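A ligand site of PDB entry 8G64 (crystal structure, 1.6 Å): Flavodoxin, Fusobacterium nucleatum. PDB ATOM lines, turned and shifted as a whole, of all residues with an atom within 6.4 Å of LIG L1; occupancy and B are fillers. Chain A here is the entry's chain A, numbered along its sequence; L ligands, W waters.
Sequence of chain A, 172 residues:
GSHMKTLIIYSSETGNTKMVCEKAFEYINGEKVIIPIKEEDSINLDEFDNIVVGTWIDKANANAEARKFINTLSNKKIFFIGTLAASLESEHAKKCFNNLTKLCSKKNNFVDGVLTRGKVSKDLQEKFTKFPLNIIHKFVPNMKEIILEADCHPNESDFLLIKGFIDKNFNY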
ATOM      1  N   SER A  11     -27.148   3.289  -7.499  1.00  0.00           N
ATOM      2  CA  SER A  11     -25.908   3.664  -8.152  1.00  0.00           C
ATOM      3  C   SER A  11     -24.784   3.491  -7.138  1.00  0.00           C
ATOM      4  O   SER A  11     -24.942   3.848  -5.968  1.00  0.00           O
ATOM      5  CB  SER A  11     -25.921   5.127  -8.611  1.00  0.00           C
ATOM      6  OG  SER A  11     -26.896   5.375  -9.574  1.00  0.00           O
ATOM      7  N   SER A  12     -23.628   3.022  -7.593  1.00  0.00           N
ATOM      8  CA  SER A  12     -22.448   2.972  -6.748  1.00  0.00           C
ATOM      9  C   SER A  12     -21.222   2.845  -7.646  1.00  0.00           C
ATOM     10  O   SER A  12     -21.169   1.948  -8.491  1.00  0.00           O
ATOM     11  CB  SER A  12     -22.509   1.791  -5.767  1.00  0.00           C
ATOM     12  OG  SER A  12     -21.453   1.845  -4.810  1.00  0.00           O
ATOM     13  N   GLU A  13     -20.262   3.738  -7.466  1.00  0.00           N
ATOM     14  CA  GLU A  13     -19.005   3.673  -8.201  1.00  0.00           C
ATOM     15  C   GLU A  13     -17.895   2.963  -7.423  1.00  0.00           C
ATOM     16  O   GLU A  13     -17.189   2.128  -8.001  1.00  0.00           O
ATOM     17  CB  GLU A  13     -18.531   5.072  -8.577  1.00  0.00           C
ATOM     18  CG  GLU A  13     -19.381   5.733  -9.657  1.00  0.00           C
ATOM     19  CD  GLU A  13     -19.248   5.042 -11.008  1.00  0.00           C
ATOM     20  OE1 GLU A  13     -20.281   4.895 -11.700  1.00  0.00           O
ATOM     21  OE2 GLU A  13     -18.118   4.654 -11.371  1.00  0.00           O
ATOM     22  N   THR A  14     -17.750   3.274  -6.138  1.00  0.00           N
ATOM     23  CA  THR A  14     -16.704   2.661  -5.325  1.00  0.00           C
ATOM     24  C   THR A  14     -17.267   1.749  -4.228  1.00  0.00           C
ATOM     25  O   THR A  14     -16.509   1.303  -3.358  1.00  0.00           O
ATOM     26  CB  THR A  14     -15.793   3.711  -4.710  1.00  0.00           C
ATOM     27  OG1 THR A  14     -16.534   4.826  -4.206  1.00  0.00           O
ATOM     28  CG2 THR A  14     -14.804   4.230  -5.758  1.00  0.00           C
ATOM     29  N   GLY A  15     -18.552   1.419  -4.302  1.00  0.00           N
ATOM     30  CA  GLY A  15     -19.129   0.359  -3.508  1.00  0.00           C
ATOM     31  C   GLY A  15     -19.785   0.775  -2.206  1.00  0.00           C
ATOM     32  O   GLY A  15     -20.428  -0.068  -1.561  1.00  0.00           O
ATOM     33  N   ASN A  16     -19.628   2.036  -1.786  1.00  0.00           N
ATOM     34  CA  ASN A  16     -20.188   2.413  -0.489  1.00  0.00           C
ATOM     35  C   ASN A  16     -21.723   2.319  -0.503  1.00  0.00           C
ATOM     36  O   ASN A  16     -22.332   1.775   0.421  1.00  0.00           O
ATOM     37  CB  ASN A  16     -19.769   3.830  -0.113  1.00  0.00           C
ATOM     38  CG  ASN A  16     -18.287   4.013   0.023  1.00  0.00           C
ATOM     39  OD1 ASN A  16     -17.528   3.072   0.282  1.00  0.00           O
ATOM     40  ND2 ASN A  16     -17.860   5.259  -0.127  1.00  0.00           N
ATOM     41  N   THR A  17     -22.336   2.894  -1.532  1.00  0.00           N
ATOM     42  CA  THR A  17     -23.803   2.883  -1.631  1.00  0.00           C
ATOM     43  C   THR A  17     -24.309   1.457  -1.809  1.00  0.00           C
ATOM     44  O   THR A  17     -25.319   1.079  -1.216  1.00  0.00           O
ATOM     45  CB  THR A  17     -24.233   3.789  -2.796  1.00  0.00           C
ATOM     46  OG1 THR A  17     -23.580   5.061  -2.645  1.00  0.00           O
ATOM     47  CG2 THR A  17     -25.722   3.985  -2.796  1.00  0.00           C
ATOM     48  N   LYS A  18     -23.611   0.652  -2.619  1.00  0.00           N
ATOM     49  CA  LYS A  18     -23.988  -0.747  -2.737  1.00  0.00           C
ATOM     50  C   LYS A  18     -23.986  -1.415  -1.375  1.00  0.00           C
ATOM     51  O   LYS A  18     -24.910  -2.160  -1.039  1.00  0.00           O
ATOM     52  CB  LYS A  18     -23.043  -1.456  -3.695  1.00  0.00           C
ATOM     53  CG  LYS A  18     -23.374  -2.910  -3.912  1.00  0.00           C
ATOM     54  CD  LYS A  18     -22.405  -3.566  -4.888  1.00  0.00           C
ATOM     55  CE  LYS A  18     -22.767  -5.051  -5.058  1.00  0.00           C
ATOM     56  NZ  LYS A  18     -21.819  -5.739  -5.985  1.00  0.00           N
ATOM     57  N   THR A  55     -28.209   6.236  -3.843  1.00  0.00           N
ATOM     58  CA  THR A  55     -27.486   7.276  -4.558  1.00  0.00           C
ATOM     59  C   THR A  55     -26.278   7.722  -3.742  1.00  0.00           C
ATOM     60  O   THR A  55     -26.303   7.697  -2.507  1.00  0.00           O
ATOM     61  CB  THR A  55     -28.419   8.479  -4.862  1.00  0.00           C
ATOM     62  OG1 THR A  55     -27.741   9.511  -5.601  1.00  0.00           O
ATOM     63  CG2 THR A  55     -28.966   9.098  -3.577  1.00  0.00           C
ATOM     64  N   TRP A  56     -25.213   8.090  -4.437  1.00  0.00           N
ATOM     65  CA  TRP A  56     -24.108   8.769  -3.794  1.00  0.00           C
ATOM     66  C   TRP A  56     -24.159  10.265  -4.095  1.00  0.00           C
ATOM     67  O   TRP A  56     -24.566  10.685  -5.182  1.00  0.00           O
ATOM     68  CB  TRP A  56     -22.734   8.179  -4.194  1.00  0.00           C
ATOM     69  CG  TRP A  56     -22.505   7.987  -5.645  1.00  0.00           C
ATOM     70  CD1 TRP A  56     -22.899   6.926  -6.401  1.00  0.00           C
ATOM     71  CD2 TRP A  56     -21.759   8.858  -6.508  1.00  0.00           C
ATOM     72  NE1 TRP A  56     -22.476   7.096  -7.689  1.00  0.00           N
ATOM     73  CE2 TRP A  56     -21.772   8.271  -7.784  1.00  0.00           C
ATOM     74  CE3 TRP A  56     -21.110  10.079  -6.335  1.00  0.00           C
ATOM     75  CZ2 TRP A  56     -21.144   8.860  -8.884  1.00  0.00           C
ATOM     76  CZ3 TRP A  56     -20.494  10.685  -7.430  1.00  0.00           C
ATOM     77  CH2 TRP A  56     -20.520  10.069  -8.687  1.00  0.00           C
ATOM     78  N   ILE A  57     -23.743  11.070  -3.127  1.00  0.00           N
ATOM     79  CA  ILE A  57     -23.792  12.517  -3.260  1.00  0.00           C
ATOM     80  C   ILE A  57     -22.663  12.987  -4.153  1.00  0.00           C
ATOM     81  O   ILE A  57     -21.498  12.607  -3.967  1.00  0.00           O
ATOM     82  CB  ILE A  57     -23.725  13.191  -1.883  1.00  0.00           C
ATOM     83  CG1 ILE A  57     -25.014  12.934  -1.128  1.00  0.00           C
ATOM     84  CG2 ILE A  57     -23.458  14.680  -2.050  1.00  0.00           C
ATOM     85  CD1 ILE A  57     -26.283  13.484  -1.818  1.00  0.00           C
ATOM     86  N   ASP A  58     -23.019  13.814  -5.135  1.00  0.00           N
ATOM     87  CA  ASP A  58     -22.106  14.461  -6.061  1.00  0.00           C
ATOM     88  C   ASP A  58     -22.451  15.951  -6.034  1.00  0.00           C
ATOM     89  O   ASP A  58     -23.521  16.358  -6.495  1.00  0.00           O
ATOM     90  CB  ASP A  58     -22.261  13.863  -7.471  1.00  0.00           C
ATOM     91  CG  ASP A  58     -21.302  14.465  -8.492  1.00  0.00           C
ATOM     92  OD1 ASP A  58     -20.704  15.521  -8.208  1.00  0.00           O
ATOM     93  OD2 ASP A  58     -21.174  13.882  -9.582  1.00  0.00           O
ATOM     94  N   LYS A  59     -21.571  16.767  -5.464  1.00  0.00           N
ATOM     95  CA  LYS A  59     -21.800  18.209  -5.353  1.00  0.00           C
ATOM     96  C   LYS A  59     -23.156  18.513  -4.722  1.00  0.00           C
ATOM     97  O   LYS A  59     -23.979  19.273  -5.242  1.00  0.00           O
ATOM     98  CB  LYS A  59     -21.691  18.924  -6.716  1.00  0.00           C
ATOM     99  CG  LYS A  59     -20.361  18.843  -7.408  1.00  0.00           C
ATOM    100  CD  LYS A  59     -20.481  19.378  -8.858  1.00  0.00           C
ATOM    101  CE  LYS A  59     -20.791  18.273  -9.877  1.00  0.00           C
ATOM    102  NZ  LYS A  59     -19.627  17.390 -10.164  1.00  0.00           N
ATOM    103  N   ALA A  60     -23.394  17.891  -3.571  1.00  0.00           N
ATOM    104  CA  ALA A  60     -24.578  18.076  -2.729  1.00  0.00           C
ATOM    105  C   ALA A  60     -25.864  17.530  -3.327  1.00  0.00           C
ATOM    106  O   ALA A  60     -26.950  17.793  -2.784  1.00  0.00           O
ATOM    107  CB  ALA A  60     -24.795  19.549  -2.374  1.00  0.00           C
ATOM    108  N   ASN A  61     -25.792  16.754  -4.406  1.00  0.00           N
ATOM    109  CA  ASN A  61     -26.994  16.283  -5.066  1.00  0.00           C
ATOM    110  C   ASN A  61     -26.844  14.812  -5.446  1.00  0.00           C
ATOM    111  O   ASN A  61     -25.746  14.252  -5.380  1.00  0.00           O
ATOM    112  CB  ASN A  61     -27.298  17.107  -6.312  1.00  0.00           C
ATOM    113  CG  ASN A  61     -27.984  18.402  -5.988  1.00  0.00           C
ATOM    114  OD1 ASN A  61     -29.217  18.448  -5.870  1.00  0.00           O
ATOM    115  ND2 ASN A  61     -27.208  19.472  -5.801  1.00  0.00           N
ATOM    116  N   THR A  83     -25.279   7.870   0.344  1.00  0.00           N
ATOM    117  CA  THR A  83     -23.988   7.968   0.997  1.00  0.00           C
ATOM    118  C   THR A  83     -23.282   9.253   0.573  1.00  0.00           C
ATOM    119  O   THR A  83     -23.482   9.760  -0.534  1.00  0.00           O
ATOM    120  CB  THR A  83     -23.073   6.768   0.728  1.00  0.00           C
ATOM    121  OG1 THR A  83     -22.642   6.736  -0.648  1.00  0.00           O
ATOM    122  CG2 THR A  83     -23.806   5.450   1.057  1.00  0.00           C
ATOM    123  N   LEU A  84     -22.508   9.804   1.509  1.00  0.00           N
ATOM    124  CA  LEU A  84     -21.700  10.989   1.276  1.00  0.00           C
ATOM    125  C   LEU A  84     -20.539  10.934   2.246  1.00  0.00           C
ATOM    126  O   LEU A  84     -20.566  10.198   3.224  1.00  0.00           O
ATOM    127  CB  LEU A  84     -22.508  12.273   1.470  1.00  0.00           C
ATOM    128  CG  LEU A  84     -22.834  12.708   2.897  1.00  0.00           C
ATOM    129  CD1 LEU A  84     -23.353  14.147   2.887  1.00  0.00           C
ATOM    130  CD2 LEU A  84     -23.876  11.792   3.545  1.00  0.00           C
ATOM    131  N   ALA A  85     -19.500  11.732   1.978  1.00  0.00           N
ATOM    132  CA  ALA A  85     -18.313  11.723   2.830  1.00  0.00           C
ATOM    133  C   ALA A  85     -18.380  12.710   3.982  1.00  0.00           C
ATOM    134  O   ALA A  85     -17.652  12.550   4.969  1.00  0.00           O
ATOM    135  CB  ALA A  85     -17.065  11.998   1.985  1.00  0.00           C
ATOM    136  N   ALA A  86     -19.211  13.746   3.876  1.00  0.00           N
ATOM    137  CA  ALA A  86     -19.307  14.731   4.933  1.00  0.00           C
ATOM    138  C   ALA A  86     -19.835  14.106   6.227  1.00  0.00           C
ATOM    139  O   ALA A  86     -20.460  13.039   6.229  1.00  0.00           O
ATOM    140  CB  ALA A  86     -20.234  15.865   4.527  1.00  0.00           C
ATOM    141  N   SER A  87     -19.612  14.813   7.334  1.00  0.00           N
ATOM    142  CA  SER A  87     -20.205  14.382   8.602  1.00  0.00           C
ATOM    143  C   SER A  87     -21.726  14.371   8.513  1.00  0.00           C
ATOM    144  O   SER A  87     -22.338  15.282   7.946  1.00  0.00           O
ATOM    145  CB  SER A  87     -19.769  15.315   9.723  1.00  0.00           C
ATOM    146  OG  SER A  87     -20.548  15.037  10.889  1.00  0.00           O
ATOM    147  N   HIS A  92     -23.945  20.664   5.592  1.00  0.00           N
ATOM    148  CA  HIS A  92     -23.850  20.103   4.252  1.00  0.00           C
ATOM    149  C   HIS A  92     -24.724  18.861   4.119  1.00  0.00           C
ATOM    150  O   HIS A  92     -25.475  18.712   3.148  1.00  0.00           O
ATOM    151  CB  HIS A  92     -22.397  19.772   3.906  1.00  0.00           C
ATOM    152  CG  HIS A  92     -22.193  19.215   2.536  1.00  0.00           C
ATOM    153  ND1 HIS A  92     -22.162  20.007   1.406  1.00  0.00           N
ATOM    154  CD2 HIS A  92     -21.999  17.947   2.113  1.00  0.00           C
ATOM    155  CE1 HIS A  92     -21.953  19.249   0.353  1.00  0.00           C
ATOM    156  NE2 HIS A  92     -21.881  17.991   0.741  1.00  0.00           N
ATOM    157  N   CYS A  96     -27.856  18.208   1.611  1.00  0.00           N
ATOM    158  CA  CYS A  96     -27.982  17.040   0.740  1.00  0.00           C
ATOM    159  C   CYS A  96     -29.314  16.336   0.969  1.00  0.00           C
ATOM    160  O   CYS A  96     -29.985  15.925   0.012  1.00  0.00           O
ATOM    161  CB  CYS A  96     -26.851  16.051   0.997  1.00  0.00           C
ATOM    162  SG  CYS A  96     -25.197  16.636   0.561  1.00  0.00           S
ATOM    163  N   THR A 116     -26.062   7.960   4.967  1.00  0.00           N
ATOM    164  CA  THR A 116     -24.994   7.253   5.661  1.00  0.00           C
ATOM    165  C   THR A 116     -23.680   7.774   5.103  1.00  0.00           C
ATOM    166  O   THR A 116     -23.632   8.422   4.052  1.00  0.00           O
ATOM    167  CB  THR A 116     -25.081   5.725   5.468  1.00  0.00           C
ATOM    168  OG1 THR A 116     -25.128   5.449   4.066  1.00  0.00           O
ATOM    169  CG2 THR A 116     -26.354   5.165   6.118  1.00  0.00           C
ATOM    170  N   ARG A 117     -22.593   7.515   5.812  1.00  0.00           N
ATOM    171  CA  ARG A 117     -21.301   8.055   5.433  1.00  0.00           C
ATOM    172  C   ARG A 117     -20.521   7.035   4.623  1.00  0.00           C
ATOM    173  O   ARG A 117     -20.652   5.821   4.819  1.00  0.00           O
ATOM    174  CB  ARG A 117     -20.512   8.440   6.680  1.00  0.00           C
ATOM    175  CG  ARG A 117     -19.424   9.465   6.425  1.00  0.00           C
ATOM    176  CD  ARG A 117     -19.061  10.204   7.673  1.00  0.00           C
ATOM    177  NE  ARG A 117     -17.999  11.182   7.448  1.00  0.00           N
ATOM    178  CZ  ARG A 117     -17.436  11.886   8.420  1.00  0.00           C
ATOM    179  NH1 ARG A 117     -17.809  11.736   9.671  1.00  0.00           N
ATOM    180  NH2 ARG A 117     -16.477  12.758   8.130  1.00  0.00           N
ATOM    181  N   GLY A 118     -19.695   7.541   3.699  1.00  0.00           N
ATOM    182  CA  GLY A 118     -18.875   6.699   2.858  1.00  0.00           C
ATOM    183  C   GLY A 118     -17.547   7.343   2.528  1.00  0.00           C
ATOM    184  O   GLY A 118     -17.505   8.522   2.189  1.00  0.00           O
ATOM    185  N   LYS A 119     -16.481   6.562   2.632  1.00  0.00           N
ATOM    186  CA  LYS A 119     -15.132   7.055   2.368  1.00  0.00           C
ATOM    187  C   LYS A 119     -15.016   7.701   0.991  1.00  0.00           C
ATOM    188  O   LYS A 119     -15.675   7.306   0.020  1.00  0.00           O
ATOM    189  CB  LYS A 119     -14.132   5.913   2.469  1.00  0.00           C
ATOM    190  CG  LYS A 119     -14.306   4.823   1.399  1.00  0.00           C
ATOM    191  CD  LYS A 119     -13.459   3.594   1.684  1.00  0.00           C
ATOM    192  CE  LYS A 119     -14.162   2.670   2.679  1.00  0.00           C
ATOM    193  NZ  LYS A 119     -15.349   1.964   2.084  1.00  0.00           N
ATOM    194  N   VAL A 120     -14.110   8.674   0.904  1.00  0.00           N
ATOM    195  CA  VAL A 120     -13.732   9.291  -0.360  1.00  0.00           C
ATOM    196  C   VAL A 120     -12.778   8.353  -1.099  1.00  0.00           C
ATOM    197  O   VAL A 120     -11.837   7.805  -0.503  1.00  0.00           O
ATOM    198  CB  VAL A 120     -13.086  10.667  -0.115  1.00  0.00           C
ATOM    199  CG1 VAL A 120     -12.742  11.342  -1.463  1.00  0.00           C
ATOM    200  CG2 VAL A 120     -13.993  11.559   0.737  1.00  0.00           C
ATOM    201  N   SER A 121     -13.020   8.170  -2.387  1.00  0.00           N
ATOM    202  CA  SER A 121     -12.210   7.239  -3.167  1.00  0.00           C
ATOM    203  C   SER A 121     -10.757   7.695  -3.171  1.00  0.00           C
ATOM    204  O   SER A 121     -10.447   8.869  -2.991  1.00  0.00           O
ATOM    205  CB  SER A 121     -12.718   7.153  -4.607  1.00  0.00           C
ATOM    206  OG  SER A 121     -12.390   8.338  -5.330  1.00  0.00           O
ATOM    207  N   LEU A 124     -10.199  10.357  -5.807  1.00  0.00           N
ATOM    208  CA  LEU A 124     -10.702  11.696  -5.480  1.00  0.00           C
ATOM    209  C   LEU A 124      -9.858  12.337  -4.383  1.00  0.00           C
ATOM    210  O   LEU A 124      -9.612  13.547  -4.412  1.00  0.00           O
ATOM    211  CB  LEU A 124     -12.164  11.629  -5.073  1.00  0.00           C
ATOM    212  CG  LEU A 124     -12.861  12.933  -4.747  1.00  0.00           C
ATOM    213  CD1 LEU A 124     -12.668  13.962  -5.825  1.00  0.00           C
ATOM    214  CD2 LEU A 124     -14.348  12.647  -4.542  1.00  0.00           C
ATOM    215  N   HIS A 137     -12.276  24.115  -2.602  1.00  0.00           N
ATOM    216  CA  HIS A 137     -12.562  23.774  -1.209  1.00  0.00           C
ATOM    217  C   HIS A 137     -11.632  24.454  -0.220  1.00  0.00           C
ATOM    218  O   HIS A 137     -11.640  24.108   0.959  1.00  0.00           O
ATOM    219  CB  HIS A 137     -12.504  22.265  -1.021  1.00  0.00           C
ATOM    220  CG  HIS A 137     -13.549  21.540  -1.779  1.00  0.00           C
ATOM    221  ND1 HIS A 137     -13.384  21.176  -3.103  1.00  0.00           N
ATOM    222  CD2 HIS A 137     -14.798  21.146  -1.431  1.00  0.00           C
ATOM    223  CE1 HIS A 137     -14.472  20.570  -3.528  1.00  0.00           C
ATOM    224  NE2 HIS A 137     -15.344  20.537  -2.538  1.00  0.00           N
ATOM    225  N   ILE A 146     -12.582  15.950   7.680  1.00  0.00           N
ATOM    226  CA  ILE A 146     -13.796  15.351   7.132  1.00  0.00           C
ATOM    227  C   ILE A 146     -13.438  14.148   6.266  1.00  0.00           C
ATOM    228  O   ILE A 146     -14.053  13.081   6.358  1.00  0.00           O
ATOM    229  CB  ILE A 146     -14.606  16.384   6.338  1.00  0.00           C
ATOM    230  CG1 ILE A 146     -15.223  17.408   7.284  1.00  0.00           C
ATOM    231  CG2 ILE A 146     -15.675  15.673   5.504  1.00  0.00           C
ATOM    232  CD1 ILE A 146     -15.701  18.657   6.573  1.00  0.00           C
ATOM    233  N   PRO A 154     -18.501   3.045   4.774  1.00  0.00           N
ATOM    234  CA  PRO A 154     -19.560   2.697   5.741  1.00  0.00           C
ATOM    235  C   PRO A 154     -19.094   1.643   6.735  1.00  0.00           C
ATOM    236  O   PRO A 154     -18.286   0.752   6.432  1.00  0.00           O
ATOM    237  CB  PRO A 154     -20.694   2.158   4.850  1.00  0.00           C
ATOM    238  CG  PRO A 154     -20.368   2.607   3.442  1.00  0.00           C
ATOM    239  CD  PRO A 154     -18.860   2.628   3.412  1.00  0.00           C
HETATM  240  N1  LIG L   1     -19.387  13.815  -0.546  1.00  0.00           N
HETATM  241  C1  LIG L   1     -19.994  14.825   0.145  1.00  0.00           C
HETATM  242  O1  LIG L   1     -20.175  14.759   1.351  1.00  0.00           O
HETATM  243  N2  LIG L   1     -20.439  15.924  -0.553  1.00  0.00           N
HETATM  244  C2  LIG L   1     -20.221  16.063  -1.887  1.00  0.00           C
HETATM  245  O2  LIG L   1     -20.664  17.081  -2.451  1.00  0.00           O
HETATM  246  C3  LIG L   1     -19.596  15.041  -2.568  1.00  0.00           C
HETATM  247  N3  LIG L   1     -19.380  15.146  -3.927  1.00  0.00           N
HETATM  248  C4  LIG L   1     -18.757  14.120  -4.598  1.00  0.00           C
HETATM  249  C5  LIG L   1     -18.549  14.228  -5.969  1.00  0.00           C
HETATM  250  C6  LIG L   1     -17.932  13.196  -6.655  1.00  0.00           C
HETATM  251  C7  LIG L   1     -17.719  13.324  -8.137  1.00  0.00           C
HETATM  252  C8  LIG L   1     -17.490  12.063  -5.982  1.00  0.00           C
HETATM  253  C9  LIG L   1     -16.833  10.930  -6.732  1.00  0.00           C
HETATM  254  C10 LIG L   1     -17.707  11.954  -4.614  1.00  0.00           C
HETATM  255  C11 LIG L   1     -18.326  12.983  -3.918  1.00  0.00           C
HETATM  256  N4  LIG L   1     -18.544  12.874  -2.550  1.00  0.00           N
HETATM  257  C12 LIG L   1     -19.175  13.904  -1.890  1.00  0.00           C
HETATM  258  C13 LIG L   1     -18.146  11.645  -1.804  1.00  0.00           C
HETATM  259  C14 LIG L   1     -19.168  10.535  -2.116  1.00  0.00           C
HETATM  260  O3  LIG L   1     -20.507  10.986  -1.972  1.00  0.00           O
HETATM  261  C15 LIG L   1     -18.977   9.312  -1.194  1.00  0.00           C
HETATM  262  O4  LIG L   1     -17.590   8.981  -1.215  1.00  0.00           O
HETATM  263  C16 LIG L   1     -19.841   8.136  -1.596  1.00  0.00           C
HETATM  264  O5  LIG L   1     -19.990   7.296  -0.434  1.00  0.00           O
HETATM  265  C17 LIG L   1     -19.316   7.318  -2.755  1.00  0.00           C
HETATM  266  O6  LIG L   1     -20.310   6.351  -3.125  1.00  0.00           O
HETATM  267  P1  LIG L   1     -19.990   5.026  -3.937  1.00  0.00           P
HETATM  268  O7  LIG L   1     -19.624   5.467  -5.340  1.00  0.00           O
HETATM  269  O8  LIG L   1     -18.821   4.331  -3.239  1.00  0.00           O
HETATM  270  O9  LIG L   1     -21.276   4.228  -3.845  1.00  0.00           O
HETATM  271  C1  LG2 L   2     -18.355  23.142  -1.916  1.00  0.00           C
HETATM  272  C2  LG2 L   2     -17.511  20.726  -6.048  1.00  0.00           C
HETATM  273  C3  LG2 L   2     -16.297  16.809  -3.468  1.00  0.00           C
HETATM  274  C4  LG2 L   2     -17.806  18.983   0.563  1.00  0.00           C
HETATM  275  C5  LG2 L   2     -18.200  22.835  -3.253  1.00  0.00           C
HETATM  276  C6  LG2 L   2     -18.355  23.756  -4.363  1.00  0.00           C
HETATM  277  C7  LG2 L   2     -18.119  23.097  -5.502  1.00  0.00           C
HETATM  278  C8  LG2 L   2     -17.824  21.725  -5.164  1.00  0.00           C
HETATM  279  C9  LG2 L   2     -18.167  23.630  -6.949  1.00  0.00           C
HETATM  280  C10 LG2 L   2     -18.728  25.253  -4.219  1.00  0.00           C
HETATM  281  C11 LG2 L   2     -20.241  25.406  -4.197  1.00  0.00           C
HETATM  282  C12 LG2 L   2     -20.789  25.323  -5.602  1.00  0.00           C
HETATM  283  O1  LG2 L   2     -21.647  24.441  -5.864  1.00  0.00           O
HETATM  284  O2  LG2 L   2     -20.358  26.125  -6.474  1.00  0.00           O
HETATM  285  C13 LG2 L   2     -17.097  19.455  -5.710  1.00  0.00           C
HETATM  286  C14 LG2 L   2     -16.654  18.428  -6.619  1.00  0.00           C
HETATM  287  C15 LG2 L   2     -16.325  17.342  -5.909  1.00  0.00           C
HETATM  288  C16 LG2 L   2     -16.524  17.667  -4.519  1.00  0.00           C
HETATM  289  C17 LG2 L   2     -16.636  18.615  -8.154  1.00  0.00           C
HETATM  290  C18 LG2 L   2     -15.776  15.989  -6.385  1.00  0.00           C
HETATM  291  C19 LG2 L   2     -15.314  15.824  -7.653  1.00  0.00           C
HETATM  292  C20 LG2 L   2     -16.628  17.061  -2.159  1.00  0.00           C
HETATM  293  C21 LG2 L   2     -16.478  16.102  -1.065  1.00  0.00           C
HETATM  294  C22 LG2 L   2     -16.911  16.714   0.045  1.00  0.00           C
HETATM  295  C23 LG2 L   2     -17.325  18.042  -0.303  1.00  0.00           C
HETATM  296  C24 LG2 L   2     -15.903  14.676  -1.246  1.00  0.00           C
HETATM  297  C25 LG2 L   2     -16.963  16.170   1.487  1.00  0.00           C
HETATM  298  C26 LG2 L   2     -16.152  15.177   1.879  1.00  0.00           C
HETATM  299  C27 LG2 L   2     -18.076  20.297   0.219  1.00  0.00           C
HETATM  300  C28 LG2 L   2     -18.534  21.303   1.150  1.00  0.00           C
HETATM  301  C29 LG2 L   2     -18.711  22.445   0.485  1.00  0.00           C
HETATM  302  C30 LG2 L   2     -18.322  22.205  -0.895  1.00  0.00           C
HETATM  303  C31 LG2 L   2     -18.815  21.057   2.636  1.00  0.00           C
HETATM  304  C32 LG2 L   2     -19.203  23.788   1.068  1.00  0.00           C
HETATM  305  C33 LG2 L   2     -20.576  24.122   0.468  1.00  0.00           C
HETATM  306  C34 LG2 L   2     -21.621  23.153   0.964  1.00  0.00           C
HETATM  307  O3  LG2 L   2     -21.782  22.986   2.190  1.00  0.00           O
HETATM  308  O4  LG2 L   2     -22.327  22.548   0.142  1.00  0.00           O
HETATM  309  N1  LG2 L   2     -17.848  21.616  -3.786  1.00  0.00           N
HETATM  310  N2  LG2 L   2     -17.012  18.964  -4.424  1.00  0.00           N
HETATM  311  N3  LG2 L   2     -17.148  18.221  -1.642  1.00  0.00           N
HETATM  312  N4  LG2 L   2     -17.951  20.864  -1.055  1.00  0.00           N
HETATM  313 FE1  LG2 L   2     -17.472  19.972  -2.704  1.00  0.00          FE
HETATM  314  O   HOH W   1     -15.670   9.120  -3.303  1.00  0.00           O
HETATM  315  O   HOH W   2     -18.817   7.669  -6.391  1.00  0.00           O
HETATM  316  O   HOH W   3     -19.575  19.480  -2.946  1.00  0.00           O
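The backbone NH (N) of Thr 14 lies within hydrogen-bond range of an oxygen (O7) of LIG L1 (3.0 Å).
OG1 of Thr 14 is in hydrogen-bond range of O8 of LIG L1 (2.5 Å).
An oxygen (O9) of LIG L1 lies within hydrogen-bond range of the side-chain hydroxyl (OG) of Ser 12 (2.6 Å).
OG1 of Thr 83 lies within hydrogen-bond range of O5 of LIG L1 (2.7 Å).
N of Thr 17 lies within hydrogen-bond range of O9 of LIG L1, at 2.9 Å.
OG1 of Thr 17 lies within hydrogen-bond range of O9 of LIG L1 (2.7 Å).
N of Ile 57 sits at hydrogen-bond distance from O3 of LIG L1 (3.4 Å).
An oxygen (O3) of LIG L1 sits at hydrogen-bond distance from the backbone carbonyl oxygen (O) of Ile 57 (2.8 Å).
The backbone NH (N) of Glu 13 sits at hydrogen-bond distance from an oxygen (O7) of LIG L1, at 2.8 Å.
The backbone carbonyl oxygen (O) of Lys 119 sits at hydrogen-bond distance from an oxygen (O4) of LIG L1.
A ring nitrogen (NE2) of His 92 sits at hydrogen-bond distance from a nitrogen (N2) of LIG L1 (2.8 Å).
N of Asn 16 lies within hydrogen-bond range of O8 of LIG L1 (2.8 Å).
ND2 of Asn 16 is in hydrogen-bond range of O5 of LIG L1 (3.0 Å).
N of Ala 86 sits at hydrogen-bond distance from O1 of LIG L1, 2.9 Å away.
An oxygen (O2) of LIG L1 is in hydrogen-bond range of the backbone NH (N) of Ala 60 (3.1 Å).
An oxygen (O8) of LIG L1 lies within hydrogen-bond range of the backbone NH (N) of Gly 15 (3.1 Å).
The backbone NH (N) of Lys 59 lies within hydrogen-bond range of a nitrogen (N3) of LIG L1, 3.1 Å away.
N of Ala 85 lies within hydrogen-bond range of O1 of LIG L1.
O of Gly 118 lies within hydrogen-bond range of O4 of LIG L1.
A ring nitrogen (ND1) of His 92 lies within hydrogen-bond range of an oxygen (O4) of LG2 L2.
An iron atom (FE1) of LG2 L2 is bound by a ring nitrogen (NE2) of His 137, 2.2 Å away.
N of Lys 18 is in hydrogen-bond range of OG of Ser 12, at 3.3 Å.
The backbone NH (N) of Ile 57 sits at hydrogen-bond distance from the backbone carbonyl oxygen (O) of Thr 83 (2.9 Å).
The backbone carbonyl oxygen (O) of Thr 55 sits at hydrogen-bond distance from the backbone NH (N) of Thr 83 (3.0 Å).
The side-chain amide nitrogen (ND2) of Asn 16 sits at hydrogen-bond distance from the backbone carbonyl oxygen (O) of Lys 119 (3.0 Å).
The side-chain sulfur (SG) of Cys 96 sits at hydrogen-bond distance from the backbone carbonyl oxygen (O) of His 92, 3.3 Å away.
The side-chain amino group (NZ) of Lys 59 is in salt-bridge range of the side-chain carboxylate (OD1) of Asp 58 (2.9 Å).
The backbone carbonyl oxygen (O) of Thr 116 is in hydrogen-bond range of the backbone NH (N) of Leu 84 (3.1 Å).
The side-chain hydroxyl (OG) of Ser 121 lies within hydrogen-bond range of the backbone NH (N) of Leu 124.
Merely in contact with LIG L1: Trp 56, Asp 58, Leu 84, Leu 124 and Val 120.
Hydrophobic or aromatic side chains within 4 Å of LIG L1: Trp 56, Ile 57, Leu 84, Ala 85, Ala 86, His 92 and Leu 124.
Water W1 bridges O4 of LIG L1 (2.8 Å) and N of Ser 121 (3.0 Å).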
